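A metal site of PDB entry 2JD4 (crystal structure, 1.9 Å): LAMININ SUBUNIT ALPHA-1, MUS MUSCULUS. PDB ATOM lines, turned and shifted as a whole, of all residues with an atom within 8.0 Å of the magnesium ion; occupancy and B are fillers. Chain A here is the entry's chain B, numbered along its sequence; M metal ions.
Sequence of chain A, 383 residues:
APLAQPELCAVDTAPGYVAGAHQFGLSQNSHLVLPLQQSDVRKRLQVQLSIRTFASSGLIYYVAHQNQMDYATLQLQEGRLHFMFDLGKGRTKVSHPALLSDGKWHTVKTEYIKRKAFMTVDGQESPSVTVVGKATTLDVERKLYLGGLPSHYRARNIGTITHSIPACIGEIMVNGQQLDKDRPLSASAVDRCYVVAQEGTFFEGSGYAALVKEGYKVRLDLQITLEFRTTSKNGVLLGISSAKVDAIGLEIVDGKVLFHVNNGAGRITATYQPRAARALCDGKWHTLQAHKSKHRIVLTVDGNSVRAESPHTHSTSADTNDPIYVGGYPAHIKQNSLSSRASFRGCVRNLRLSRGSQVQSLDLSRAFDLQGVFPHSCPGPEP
The nearest printed residue that does not touch the magnesium ion is Ala 318 (4.1 Å).
The magnesium ion is bound by OD2 of Asp 319, O of Ser 317, O of Asn 263 and OD2 of Asp 246.
The side-chain amide oxygen (OD1) of Asn 263 sits at hydrogen-bond distance from the backbone NH (N) of Ala 318.
The side-chain amide nitrogen (ND2) of Asn 263 lies within hydrogen-bond range of the backbone carbonyl oxygen (O) of Ser 315 (3.2 Å).
OD1 of Asn 263 sits close to NZ of Lys 292, 3.3 Å away.
OD1 of Asp 246 lies close to N of Gly 264 (3.5 Å).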
ATOM      1  N   ARG A 219       7.020 -29.737  33.730  1.00  0.00           N
ATOM      2  CA  ARG A 219       5.738 -30.100  33.134  1.00  0.00           C
ATOM      3  C   ARG A 219       4.773 -28.944  32.845  1.00  0.00           C
ATOM      4  O   ARG A 219       5.134 -28.039  32.089  1.00  0.00           O
ATOM      5  CB  ARG A 219       5.069 -31.203  33.955  1.00  0.00           C
ATOM      6  CG  ARG A 219       5.807 -32.534  33.848  1.00  0.00           C
ATOM      7  CD  ARG A 219       5.259 -33.612  34.766  1.00  0.00           C
ATOM      8  NE  ARG A 219       3.861 -33.944  34.491  1.00  0.00           N
ATOM      9  CZ  ARG A 219       3.431 -34.622  33.435  1.00  0.00           C
ATOM     10  NH1 ARG A 219       4.294 -35.063  32.519  1.00  0.00           N
ATOM     11  NH2 ARG A 219       2.140 -34.864  33.284  1.00  0.00           N
ATOM     12  N   LEU A 220       3.585 -28.935  33.448  1.00  0.00           N
ATOM     13  CA  LEU A 220       2.606 -27.886  33.152  1.00  0.00           C
ATOM     14  C   LEU A 220       2.620 -26.567  33.931  1.00  0.00           C
ATOM     15  O   LEU A 220       2.530 -25.496  33.341  1.00  0.00           O
ATOM     16  CB  LEU A 220       1.183 -28.445  33.231  1.00  0.00           C
ATOM     17  CG  LEU A 220       0.723 -29.545  32.270  1.00  0.00           C
ATOM     18  CD1 LEU A 220      -0.727 -29.885  32.578  1.00  0.00           C
ATOM     19  CD2 LEU A 220       0.868 -29.086  30.828  1.00  0.00           C
ATOM     20  N   VAL A 245      15.354 -30.051  23.950  1.00  0.00           N
ATOM     21  CA  VAL A 245      14.593 -28.827  23.730  1.00  0.00           C
ATOM     22  C   VAL A 245      13.923 -28.211  24.967  1.00  0.00           C
ATOM     23  O   VAL A 245      14.167 -27.043  25.278  1.00  0.00           O
ATOM     24  CB  VAL A 245      13.492 -29.052  22.644  1.00  0.00           C
ATOM     25  CG1 VAL A 245      12.632 -27.803  22.488  1.00  0.00           C
ATOM     26  CG2 VAL A 245      14.149 -29.409  21.318  1.00  0.00           C
ATOM     27  N   ASP A 246      13.074 -28.986  25.641  1.00  0.00           N
ATOM     28  CA  ASP A 246      12.350 -28.509  26.819  1.00  0.00           C
ATOM     29  C   ASP A 246      13.221 -27.959  27.945  1.00  0.00           C
ATOM     30  O   ASP A 246      14.195 -28.597  28.348  1.00  0.00           O
ATOM     31  CB  ASP A 246      11.439 -29.624  27.343  1.00  0.00           C
ATOM     32  CG  ASP A 246      10.273 -29.916  26.408  1.00  0.00           C
ATOM     33  OD1 ASP A 246      10.497 -29.963  25.176  1.00  0.00           O
ATOM     34  OD2 ASP A 246       9.148 -30.096  26.890  1.00  0.00           O
ATOM     35  N   ALA A 247      12.838 -26.797  28.466  1.00  0.00           N
ATOM     36  CA  ALA A 247      13.587 -26.132  29.530  1.00  0.00           C
ATOM     37  C   ALA A 247      12.981 -24.790  29.917  1.00  0.00           C
ATOM     38  O   ALA A 247      12.202 -24.216  29.158  1.00  0.00           O
ATOM     39  CB  ALA A 247      15.036 -25.924  29.085  1.00  0.00           C
ATOM     40  N   ASN A 262      10.428 -23.125  27.158  1.00  0.00           N
ATOM     41  CA  ASN A 262      10.284 -23.868  25.911  1.00  0.00           C
ATOM     42  C   ASN A 262       9.610 -25.203  26.236  1.00  0.00           C
ATOM     43  O   ASN A 262      10.181 -26.031  26.941  1.00  0.00           O
ATOM     44  CB  ASN A 262      11.643 -24.130  25.237  1.00  0.00           C
ATOM     45  CG  ASN A 262      11.489 -24.502  23.760  1.00  0.00           C
ATOM     46  OD1 ASN A 262      10.508 -25.136  23.373  1.00  0.00           O
ATOM     47  ND2 ASN A 262      12.469 -24.118  22.936  1.00  0.00           N
ATOM     48  N   ASN A 263       8.393 -25.378  25.750  1.00  0.00           N
ATOM     49  CA  ASN A 263       7.658 -26.618  26.014  1.00  0.00           C
ATOM     50  C   ASN A 263       7.884 -27.645  24.910  1.00  0.00           C
ATOM     51  O   ASN A 263       7.341 -28.755  24.952  1.00  0.00           O
ATOM     52  CB  ASN A 263       6.156 -26.326  26.148  1.00  0.00           C
ATOM     53  CG  ASN A 263       5.827 -25.512  27.394  1.00  0.00           C
ATOM     54  OD1 ASN A 263       6.363 -25.759  28.474  1.00  0.00           O
ATOM     55  ND2 ASN A 263       4.916 -24.561  27.250  1.00  0.00           N
ATOM     56  N   GLY A 264       8.674 -27.261  23.907  1.00  0.00           N
ATOM     57  CA  GLY A 264       8.967 -28.169  22.808  1.00  0.00           C
ATOM     58  C   GLY A 264       8.754 -27.576  21.414  1.00  0.00           C
ATOM     59  O   GLY A 264       9.289 -28.085  20.432  1.00  0.00           O
ATOM     60  N   ALA A 265       7.992 -26.478  21.328  1.00  0.00           N
ATOM     61  CA  ALA A 265       7.721 -25.851  20.038  1.00  0.00           C
ATOM     62  C   ALA A 265       8.468 -24.545  19.785  1.00  0.00           C
ATOM     63  O   ALA A 265       8.322 -23.922  18.726  1.00  0.00           O
ATOM     64  CB  ALA A 265       6.222 -25.604  19.883  1.00  0.00           C
ATOM     65  N   LYS A 292       4.625 -19.894  35.181  1.00  0.00           N
ATOM     66  CA  LYS A 292       4.391 -20.647  33.959  1.00  0.00           C
ATOM     67  C   LYS A 292       3.113 -21.453  34.101  1.00  0.00           C
ATOM     68  O   LYS A 292       2.981 -22.246  35.036  1.00  0.00           O
ATOM     69  CB  LYS A 292       5.553 -21.614  33.667  1.00  0.00           C
ATOM     70  CG  LYS A 292       5.303 -22.550  32.466  1.00  0.00           C
ATOM     71  CD  LYS A 292       6.038 -23.883  32.601  1.00  0.00           C
ATOM     72  CE  LYS A 292       5.823 -24.796  31.389  1.00  0.00           C
ATOM     73  NZ  LYS A 292       4.381 -25.096  31.092  1.00  0.00           N
ATOM     74  N   HIS A 314      -0.356 -26.001  21.119  1.00  0.00           N
ATOM     75  CA  HIS A 314      -0.369 -27.445  21.352  1.00  0.00           C
ATOM     76  C   HIS A 314       0.757 -27.886  22.278  1.00  0.00           C
ATOM     77  O   HIS A 314       0.733 -28.990  22.819  1.00  0.00           O
ATOM     78  CB  HIS A 314      -0.214 -28.205  20.032  1.00  0.00           C
ATOM     79  CG  HIS A 314       1.151 -28.073  19.419  1.00  0.00           C
ATOM     80  ND1 HIS A 314       1.496 -27.029  18.596  1.00  0.00           N
ATOM     81  CD2 HIS A 314       2.272 -28.822  19.561  1.00  0.00           C
ATOM     82  CE1 HIS A 314       2.774 -27.145  18.253  1.00  0.00           C
ATOM     83  NE2 HIS A 314       3.262 -28.229  18.825  1.00  0.00           N
ATOM     84  N   SER A 315       1.745 -27.014  22.457  1.00  0.00           N
ATOM     85  CA  SER A 315       2.915 -27.300  23.292  1.00  0.00           C
ATOM     86  C   SER A 315       2.764 -26.623  24.655  1.00  0.00           C
ATOM     87  O   SER A 315       3.097 -25.441  24.797  1.00  0.00           O
ATOM     88  CB  SER A 315       4.173 -26.793  22.578  1.00  0.00           C
ATOM     89  OG  SER A 315       5.349 -27.343  23.140  1.00  0.00           O
ATOM     90  N   THR A 316       2.298 -27.379  25.647  1.00  0.00           N
ATOM     91  CA  THR A 316       2.066 -26.817  26.980  1.00  0.00           C
ATOM     92  C   THR A 316       2.855 -27.421  28.158  1.00  0.00           C
ATOM     93  O   THR A 316       2.830 -26.872  29.261  1.00  0.00           O
ATOM     94  CB  THR A 316       0.567 -26.900  27.332  1.00  0.00           C
ATOM     95  OG1 THR A 316       0.172 -28.271  27.422  1.00  0.00           O
ATOM     96  CG2 THR A 316      -0.265 -26.213  26.254  1.00  0.00           C
ATOM     97  N   SER A 317       3.538 -28.531  27.922  1.00  0.00           N
ATOM     98  CA  SER A 317       4.326 -29.187  28.977  1.00  0.00           C
ATOM     99  C   SER A 317       5.831 -29.068  28.766  1.00  0.00           C
ATOM    100  O   SER A 317       6.338 -29.324  27.672  1.00  0.00           O
ATOM    101  CB  SER A 317       3.947 -30.671  29.059  1.00  0.00           C
ATOM    102  OG  SER A 317       4.723 -31.340  30.039  1.00  0.00           O
ATOM    103  N   ALA A 318       6.549 -28.662  29.810  1.00  0.00           N
ATOM    104  CA  ALA A 318       8.010 -28.544  29.764  1.00  0.00           C
ATOM    105  C   ALA A 318       8.542 -29.853  30.355  1.00  0.00           C
ATOM    106  O   ALA A 318       8.726 -29.990  31.571  1.00  0.00           O
ATOM    107  CB  ALA A 318       8.479 -27.352  30.594  1.00  0.00           C
ATOM    108  N   ASP A 319       8.784 -30.818  29.473  1.00  0.00           N
ATOM    109  CA  ASP A 319       9.216 -32.151  29.851  1.00  0.00           C
ATOM    110  C   ASP A 319      10.684 -32.342  30.252  1.00  0.00           C
ATOM    111  O   ASP A 319      11.459 -32.986  29.545  1.00  0.00           O
ATOM    112  CB  ASP A 319       8.843 -33.110  28.717  1.00  0.00           C
ATOM    113  CG  ASP A 319       7.386 -32.946  28.306  1.00  0.00           C
ATOM    114  OD1 ASP A 319       6.513 -33.567  28.950  1.00  0.00           O
ATOM    115  OD2 ASP A 319       7.116 -32.172  27.356  1.00  0.00           O
ATOM    116  N   THR A 320      11.040 -31.791  31.404  1.00  0.00           N
ATOM    117  CA  THR A 320      12.384 -31.931  31.931  1.00  0.00           C
ATOM    118  C   THR A 320      12.395 -33.081  32.948  1.00  0.00           C
ATOM    119  O   THR A 320      11.342 -33.644  33.273  1.00  0.00           O
ATOM    120  CB  THR A 320      12.825 -30.630  32.658  1.00  0.00           C
ATOM    121  OG1 THR A 320      11.971 -30.381  33.768  1.00  0.00           O
ATOM    122  CG2 THR A 320      12.755 -29.438  31.709  1.00  0.00           C
HETATM  123 MG    MG M   1       7.107 -30.549  26.162  1.00  0.00          MG
